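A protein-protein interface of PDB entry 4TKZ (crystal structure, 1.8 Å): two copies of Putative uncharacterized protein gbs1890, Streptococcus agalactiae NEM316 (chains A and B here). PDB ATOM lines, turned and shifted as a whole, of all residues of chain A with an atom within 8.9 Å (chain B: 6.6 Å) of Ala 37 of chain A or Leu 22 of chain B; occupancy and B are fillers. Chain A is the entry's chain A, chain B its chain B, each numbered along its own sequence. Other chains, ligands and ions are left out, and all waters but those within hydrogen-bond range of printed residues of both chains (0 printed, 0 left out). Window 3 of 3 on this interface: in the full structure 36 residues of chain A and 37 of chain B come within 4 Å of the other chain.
No position is printed for both chains.
Of the 10 pairs that touch across the chains among the printed residues, none has its exchanged pair printed and touching as well.
Ala 8 of chain A touches none of the printed residues of chain B.
Of the printed residues of chain B, His 9 of chain A touches Ser 19, Leu 22 and Ile 23.
Printed residues of chain B within 4 Å of Asn 11 of chain A: Ser 18.
Printed residues of chain B within 4 Å of Phe 12 of chain A: Ser 18 and Ser 19.
Printed residues of chain B within 4 Å of Phe 35 of chain A: Leu 22.
Of chain B, only Leu 22 comes within 4 Å of Ala 37 of chain A.
Printed residues of chain A within 4 Å of Ser 19 of chain B: His 9 and Phe 12.
Leu 22 of chain B touches four residues of chain A.
The nearest printed residue of chain B that does not touch Ala 37 of chain A is Ser 18 of chain B (7.3 Å).
The nearest residue of chain A that does not touch Leu 22 of chain B is Ile 36 of chain A (4.6 Å).
The nearest printed residue of chain A that does not touch Ile 23 of chain B is Asp 63 of chain A (5.2 Å).
A ring nitrogen (ND1) of His 9 of chain A is in hydrogen-bond range of the side-chain carboxylate (OD2) of Asp 63 of chain A (2.6 Å).
N of Gly 10 of chain A is in hydrogen-bond range of O of Phe 35 of chain A (2.7 Å).
The backbone carbonyl oxygen (O) of Ala 8 of chain A sits at hydrogen-bond distance from the backbone NH (N) of Phe 35 of chain A.
Hydrophobic or aromatic side chains of chain A that line the printed part of chain B: His 9, Phe 12 and Ala 37.
Printed residues of chain B that touch a printed residue of chain A: Ser 18, Ser 19, Leu 22 and Ile 23.
Hydrophobic or aromatic side chains of chain B that line the printed part of chain A: Leu 22 and Ile 23.
Along chain B the printed residues that touch a printed residue of chain A span positions 18 to 23.
Among the printed residues, no Asp or Glu carboxylate lies within 4 Å of a Lys or Arg side-chain nitrogen of the other chain.
The side-chain hydroxyl of Ser 19 of chain B sits at hydrogen-bond distance from the backbone carbonyl oxygen of His 9 of chain A (2.6 Å).
The side-chain hydroxyl (OG) of Ser 18 of chain B sits at hydrogen-bond distance from the backbone NH (N) of Asn 11 of chain A (2.9 Å).
Among the printed residues, pairs that only touch across the chains: His 9 of chain A with Leu 22 of chain B (3.9 Å), His 9 of chain A with Ile 23 of chain B (3.9 Å), Gly 10 of chain A with Ser 18 of chain B (3.6 Å), Gly 10 of chain A with Leu 22 of chain B (3.7 Å), Phe 12 of chain A with Ser 18 of chain B (3.8 Å), Phe 12 of chain A with Ser 19 of chain B (3.1 Å), Phe 35 of chain A with Leu 22 of chain B (3.4 Å) and Ala 37 of chain A with Leu 22 of chain B (3.8 Å).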
ATOM      1  N   ALA A   8       6.070  -6.160 -14.928  1.00  0.00           N
ATOM      2  CA  ALA A   8       7.152  -5.318 -15.425  1.00  0.00           C
ATOM      3  C   ALA A   8       6.653  -4.179 -16.305  1.00  0.00           C
ATOM      4  O   ALA A   8       5.528  -4.209 -16.798  1.00  0.00           O
ATOM      5  CB  ALA A   8       8.185  -6.177 -16.182  1.00  0.00           C
ATOM      6  N   HIS A   9       7.509  -3.175 -16.480  1.00  0.00           N
ATOM      7  CA  HIS A   9       7.220  -1.997 -17.287  1.00  0.00           C
ATOM      8  C   HIS A   9       6.998  -2.323 -18.763  1.00  0.00           C
ATOM      9  O   HIS A   9       7.717  -3.141 -19.348  1.00  0.00           O
ATOM     10  CB  HIS A   9       8.385  -1.006 -17.178  1.00  0.00           C
ATOM     11  CG  HIS A   9       8.522  -0.364 -15.829  1.00  0.00           C
ATOM     12  ND1 HIS A   9       9.209  -0.955 -14.789  1.00  0.00           N
ATOM     13  CD2 HIS A   9       8.081   0.827 -15.360  1.00  0.00           C
ATOM     14  CE1 HIS A   9       9.167  -0.161 -13.731  1.00  0.00           C
ATOM     15  NE2 HIS A   9       8.495   0.928 -14.054  1.00  0.00           N
ATOM     16  N   GLY A  10       6.029  -1.649 -19.371  1.00  0.00           N
ATOM     17  CA  GLY A  10       5.707  -1.863 -20.770  1.00  0.00           C
ATOM     18  C   GLY A  10       5.183  -3.260 -21.017  1.00  0.00           C
ATOM     19  O   GLY A  10       4.512  -3.836 -20.156  1.00  0.00           O
ATOM     20  N   ASN A  11       5.483  -3.801 -22.196  1.00  0.00           N
ATOM     21  CA  ASN A  11       5.105  -5.166 -22.525  1.00  0.00           C
ATOM     22  C   ASN A  11       6.268  -6.154 -22.367  1.00  0.00           C
ATOM     23  O   ASN A  11       6.294  -7.189 -23.014  1.00  0.00           O
ATOM     24  CB  ASN A  11       4.484  -5.227 -23.927  1.00  0.00           C
ATOM     25  CG  ASN A  11       3.143  -4.495 -23.995  1.00  0.00           C
ATOM     26  OD1 ASN A  11       3.062  -3.358 -24.458  1.00  0.00           O
ATOM     27  ND2 ASN A  11       2.093  -5.141 -23.510  1.00  0.00           N
ATOM     28  N   PHE A  12       7.218  -5.807 -21.499  1.00  0.00           N
ATOM     29  CA  PHE A  12       8.269  -6.723 -21.019  1.00  0.00           C
ATOM     30  C   PHE A  12       7.668  -8.074 -20.597  1.00  0.00           C
ATOM     31  O   PHE A  12       8.185  -9.105 -21.004  1.00  0.00           O
ATOM     32  CB  PHE A  12       9.022  -6.033 -19.857  1.00  0.00           C
ATOM     33  CG  PHE A  12      10.231  -6.785 -19.283  1.00  0.00           C
ATOM     34  CD1 PHE A  12      10.165  -8.118 -18.880  1.00  0.00           C
ATOM     35  CD2 PHE A  12      11.404  -6.086 -19.032  1.00  0.00           C
ATOM     36  CE1 PHE A  12      11.264  -8.751 -18.314  1.00  0.00           C
ATOM     37  CE2 PHE A  12      12.515  -6.710 -18.472  1.00  0.00           C
ATOM     38  CZ  PHE A  12      12.442  -8.044 -18.110  1.00  0.00           C
ATOM     39  N   ASN A  34       1.291  -6.540 -17.660  1.00  0.00           N
ATOM     40  CA  ASN A  34       2.015  -5.508 -18.381  1.00  0.00           C
ATOM     41  C   ASN A  34       1.717  -4.111 -17.843  1.00  0.00           C
ATOM     42  O   ASN A  34       0.604  -3.611 -17.996  1.00  0.00           O
ATOM     43  CB  ASN A  34       1.689  -5.576 -19.879  1.00  0.00           C
ATOM     44  CG  ASN A  34       2.039  -6.923 -20.497  1.00  0.00           C
ATOM     45  OD1 ASN A  34       3.199  -7.195 -20.796  1.00  0.00           O
ATOM     46  ND2 ASN A  34       1.031  -7.761 -20.705  1.00  0.00           N
ATOM     47  N   PHE A  35       2.714  -3.492 -17.218  1.00  0.00           N
ATOM     48  CA  PHE A  35       2.577  -2.141 -16.680  1.00  0.00           C
ATOM     49  C   PHE A  35       2.843  -1.139 -17.791  1.00  0.00           C
ATOM     50  O   PHE A  35       3.957  -0.631 -17.933  1.00  0.00           O
ATOM     51  CB  PHE A  35       3.553  -1.925 -15.522  1.00  0.00           C
ATOM     52  CG  PHE A  35       3.453  -0.566 -14.876  1.00  0.00           C
ATOM     53  CD1 PHE A  35       2.213   0.004 -14.601  1.00  0.00           C
ATOM     54  CD2 PHE A  35       4.600   0.129 -14.521  1.00  0.00           C
ATOM     55  CE1 PHE A  35       2.115   1.252 -13.991  1.00  0.00           C
ATOM     56  CE2 PHE A  35       4.522   1.379 -13.909  1.00  0.00           C
ATOM     57  CZ  PHE A  35       3.269   1.946 -13.645  1.00  0.00           C
ATOM     58  N   ILE A  36       1.807  -0.851 -18.570  1.00  0.00           N
ATOM     59  CA  ILE A  36       1.967  -0.045 -19.775  1.00  0.00           C
ATOM     60  C   ILE A  36       1.662   1.425 -19.512  1.00  0.00           C
ATOM     61  O   ILE A  36       1.114   1.784 -18.466  1.00  0.00           O
ATOM     62  CB  ILE A  36       1.063  -0.558 -20.911  1.00  0.00           C
ATOM     63  CG1 ILE A  36      -0.410  -0.385 -20.533  1.00  0.00           C
ATOM     64  CG2 ILE A  36       1.369  -2.025 -21.234  1.00  0.00           C
ATOM     65  CD1 ILE A  36      -1.368  -0.723 -21.643  1.00  0.00           C
ATOM     66  N   ALA A  37       2.030   2.277 -20.463  1.00  0.00           N
ATOM     67  CA  ALA A  37       1.748   3.701 -20.360  1.00  0.00           C
ATOM     68  C   ALA A  37       0.255   3.914 -20.207  1.00  0.00           C
ATOM     69  O   ALA A  37      -0.545   3.335 -20.945  1.00  0.00           O
ATOM     70  CB  ALA A  37       2.258   4.442 -21.578  1.00  0.00           C
ATOM     71  N   GLY A  38      -0.109   4.740 -19.233  1.00  0.00           N
ATOM     72  CA  GLY A  38      -1.502   5.022 -18.947  1.00  0.00           C
ATOM     73  C   GLY A  38      -1.960   4.354 -17.667  1.00  0.00           C
ATOM     74  O   GLY A  38      -2.922   4.800 -17.040  1.00  0.00           O
ATOM     75  N   MET A  39      -1.276   3.282 -17.275  1.00  0.00           N
ATOM     76  CA  MET A  39      -1.646   2.559 -16.064  1.00  0.00           C
ATOM     77  C   MET A  39      -1.124   3.227 -14.805  1.00  0.00           C
ATOM     78  O   MET A  39       0.007   3.728 -14.768  1.00  0.00           O
ATOM     79  CB  MET A  39      -1.133   1.123 -16.107  1.00  0.00           C
ATOM     80  CG  MET A  39      -2.049   0.159 -16.812  1.00  0.00           C
ATOM     81  SD  MET A  39      -1.228  -1.443 -16.949  1.00  0.00           S
ATOM     82  CE  MET A  39      -1.372  -2.050 -15.277  1.00  0.00           C
ATOM     83  N   SER A  40      -1.959   3.234 -13.772  1.00  0.00           N
ATOM     84  CA  SER A  40      -1.569   3.747 -12.478  1.00  0.00           C
ATOM     85  C   SER A  40      -1.009   2.617 -11.633  1.00  0.00           C
ATOM     86  O   SER A  40      -1.136   1.437 -11.975  1.00  0.00           O
ATOM     87  CB  SER A  40      -2.780   4.336 -11.751  1.00  0.00           C
ATOM     88  OG  SER A  40      -3.643   3.299 -11.315  1.00  0.00           O
ATOM     89  N   ASP A  43      -3.737   0.346 -10.559  1.00  0.00           N
ATOM     90  CA  ASP A  43      -4.132  -0.587 -11.616  1.00  0.00           C
ATOM     91  C   ASP A  43      -3.335  -1.886 -11.505  1.00  0.00           C
ATOM     92  O   ASP A  43      -3.886  -2.986 -11.640  1.00  0.00           O
ATOM     93  CB  ASP A  43      -3.905   0.027 -12.996  1.00  0.00           C
ATOM     94  CG  ASP A  43      -4.883   1.130 -13.315  1.00  0.00           C
ATOM     95  OD1 ASP A  43      -5.996   1.117 -12.748  1.00  0.00           O
ATOM     96  OD2 ASP A  43      -4.535   2.002 -14.144  1.00  0.00           O
ATOM     97  N   ASP A  63      10.687  -6.540 -12.735  1.00  0.00           N
ATOM     98  CA  ASP A  63      11.833  -6.112 -13.521  1.00  0.00           C
ATOM     99  C   ASP A  63      12.919  -5.408 -12.730  1.00  0.00           C
ATOM    100  O   ASP A  63      14.096  -5.753 -12.840  1.00  0.00           O
ATOM    101  CB  ASP A  63      11.415  -5.284 -14.747  1.00  0.00           C
ATOM    102  CG  ASP A  63      10.502  -4.121 -14.415  1.00  0.00           C
ATOM    103  OD1 ASP A  63      10.050  -3.980 -13.258  1.00  0.00           O
ATOM    104  OD2 ASP A  63      10.226  -3.331 -15.344  1.00  0.00           O
ATOM    105  N   THR A  68       7.591   0.565  -9.816  1.00  0.00           N
ATOM    106  CA  THR A  68       6.183   0.335  -9.460  1.00  0.00           C
ATOM    107  C   THR A  68       5.801  -1.149  -9.370  1.00  0.00           C
ATOM    108  O   THR A  68       5.206  -1.565  -8.379  1.00  0.00           O
ATOM    109  CB  THR A  68       5.226   1.130 -10.372  1.00  0.00           C
ATOM    110  OG1 THR A  68       5.420   2.527 -10.129  1.00  0.00           O
ATOM    111  CG2 THR A  68       3.754   0.773 -10.105  1.00  0.00           C
ATOM    112  N   PRO A  69       6.152  -1.963 -10.389  1.00  0.00           N
ATOM    113  CA  PRO A  69       5.852  -3.392 -10.254  1.00  0.00           C
ATOM    114  C   PRO A  69       6.425  -4.021  -8.990  1.00  0.00           C
ATOM    115  O   PRO A  69       5.739  -4.831  -8.358  1.00  0.00           O
ATOM    116  CB  PRO A  69       6.544  -4.002 -11.486  1.00  0.00           C
ATOM    117  CG  PRO A  69       6.477  -2.935 -12.504  1.00  0.00           C
ATOM    118  CD  PRO A  69       6.677  -1.647 -11.732  1.00  0.00           C
ATOM    119  N   LEU B  17      12.707  -3.389 -24.610  1.00  0.00           N
ATOM    120  CA  LEU B  17      12.838  -2.066 -25.220  1.00  0.00           C
ATOM    121  C   LEU B  17      11.648  -1.164 -24.891  1.00  0.00           C
ATOM    122  O   LEU B  17      11.805   0.061 -24.761  1.00  0.00           O
ATOM    123  CB  LEU B  17      13.018  -2.179 -26.732  1.00  0.00           C
ATOM    124  CG  LEU B  17      14.432  -2.571 -27.162  1.00  0.00           C
ATOM    125  CD1 LEU B  17      14.488  -2.900 -28.659  1.00  0.00           C
ATOM    126  CD2 LEU B  17      15.396  -1.445 -26.800  1.00  0.00           C
ATOM    127  N   SER B  18      10.462  -1.757 -24.747  1.00  0.00           N
ATOM    128  CA  SER B  18       9.281  -0.966 -24.402  1.00  0.00           C
ATOM    129  C   SER B  18       9.364  -0.511 -22.948  1.00  0.00           C
ATOM    130  O   SER B  18       8.832   0.536 -22.604  1.00  0.00           O
ATOM    131  CB  SER B  18       7.968  -1.722 -24.671  1.00  0.00           C
ATOM    132  OG  SER B  18       7.709  -2.711 -23.693  1.00  0.00           O
ATOM    133  N   SER B  19      10.054  -1.282 -22.106  1.00  0.00           N
ATOM    134  CA  SER B  19      10.312  -0.864 -20.729  1.00  0.00           C
ATOM    135  C   SER B  19      11.195   0.380 -20.716  1.00  0.00           C
ATOM    136  O   SER B  19      10.903   1.357 -20.019  1.00  0.00           O
ATOM    137  CB  SER B  19      10.993  -1.985 -19.943  1.00  0.00           C
ATOM    138  OG  SER B  19      10.241  -3.179 -20.003  1.00  0.00           O
ATOM    139  N   LEU B  20      12.283   0.321 -21.481  1.00  0.00           N
ATOM    140  CA  LEU B  20      13.220   1.434 -21.635  1.00  0.00           C
ATOM    141  C   LEU B  20      12.524   2.694 -22.156  1.00  0.00           C
ATOM    142  O   LEU B  20      12.748   3.799 -21.650  1.00  0.00           O
ATOM    143  CB  LEU B  20      14.374   1.007 -22.566  1.00  0.00           C
ATOM    144  CG  LEU B  20      15.389   2.048 -23.046  1.00  0.00           C
ATOM    145  CD1 LEU B  20      16.106   2.668 -21.861  1.00  0.00           C
ATOM    146  CD2 LEU B  20      16.397   1.449 -24.049  1.00  0.00           C
ATOM    147  N   GLU B  21      11.668   2.521 -23.158  1.00  0.00           N
ATOM    148  CA  GLU B  21      10.934   3.633 -23.750  1.00  0.00           C
ATOM    149  C   GLU B  21       9.997   4.298 -22.734  1.00  0.00           C
ATOM    150  O   GLU B  21       9.873   5.522 -22.697  1.00  0.00           O
ATOM    151  CB  GLU B  21      10.155   3.128 -24.964  1.00  0.00           C
ATOM    152  CG  GLU B  21       8.828   3.799 -25.204  1.00  0.00           C
ATOM    153  CD  GLU B  21       8.825   4.683 -26.430  1.00  0.00           C
ATOM    154  OE1 GLU B  21       9.760   5.497 -26.594  1.00  0.00           O
ATOM    155  OE2 GLU B  21       7.876   4.563 -27.232  1.00  0.00           O
ATOM    156  N   LEU B  22       9.339   3.486 -21.914  1.00  0.00           N
ATOM    157  CA  LEU B  22       8.416   4.011 -20.896  1.00  0.00           C
ATOM    158  C   LEU B  22       9.178   4.767 -19.822  1.00  0.00           C
ATOM    159  O   LEU B  22       8.731   5.800 -19.317  1.00  0.00           O
ATOM    160  CB  LEU B  22       7.630   2.861 -20.260  1.00  0.00           C
ATOM    161  CG  LEU B  22       6.662   3.208 -19.127  1.00  0.00           C
ATOM    162  CD1 LEU B  22       5.558   4.130 -19.629  1.00  0.00           C
ATOM    163  CD2 LEU B  22       6.067   1.949 -18.487  1.00  0.00           C
ATOM    164  N   ILE B  23      10.339   4.242 -19.466  1.00  0.00           N
ATOM    165  CA  ILE B  23      11.104   4.821 -18.378  1.00  0.00           C
ATOM    166  C   ILE B  23      11.908   6.028 -18.866  1.00  0.00           C
ATOM    167  O   ILE B  23      11.833   7.107 -18.288  1.00  0.00           O
ATOM    168  CB  ILE B  23      12.005   3.756 -17.730  1.00  0.00           C
ATOM    169  CG1 ILE B  23      11.137   2.746 -16.973  1.00  0.00           C
ATOM    170  CG2 ILE B  23      13.045   4.400 -16.814  1.00  0.00           C
ATOM    171  CD1 ILE B  23      11.875   1.502 -16.526  1.00  0.00           C
ATOM    172  N   ALA B  24      12.650   5.861 -19.953  1.00  0.00           N
ATOM    173  CA  ALA B  24      13.620   6.883 -20.338  1.00  0.00           C
ATOM    174  C   ALA B  24      13.309   7.589 -21.650  1.00  0.00           C
ATOM    175  O   ALA B  24      13.962   8.577 -21.993  1.00  0.00           O
ATOM    176  CB  ALA B  24      15.017   6.283 -20.382  1.00  0.00           C
ATOM    177  N   GLY B  25      12.334   7.076 -22.393  1.00  0.00           N
ATOM    178  CA  GLY B  25      12.036   7.615 -23.705  1.00  0.00           C
ATOM    179  C   GLY B  25      12.928   6.970 -24.753  1.00  0.00           C
ATOM    180  O   GLY B  25      13.730   6.083 -24.450  1.00  0.00           O
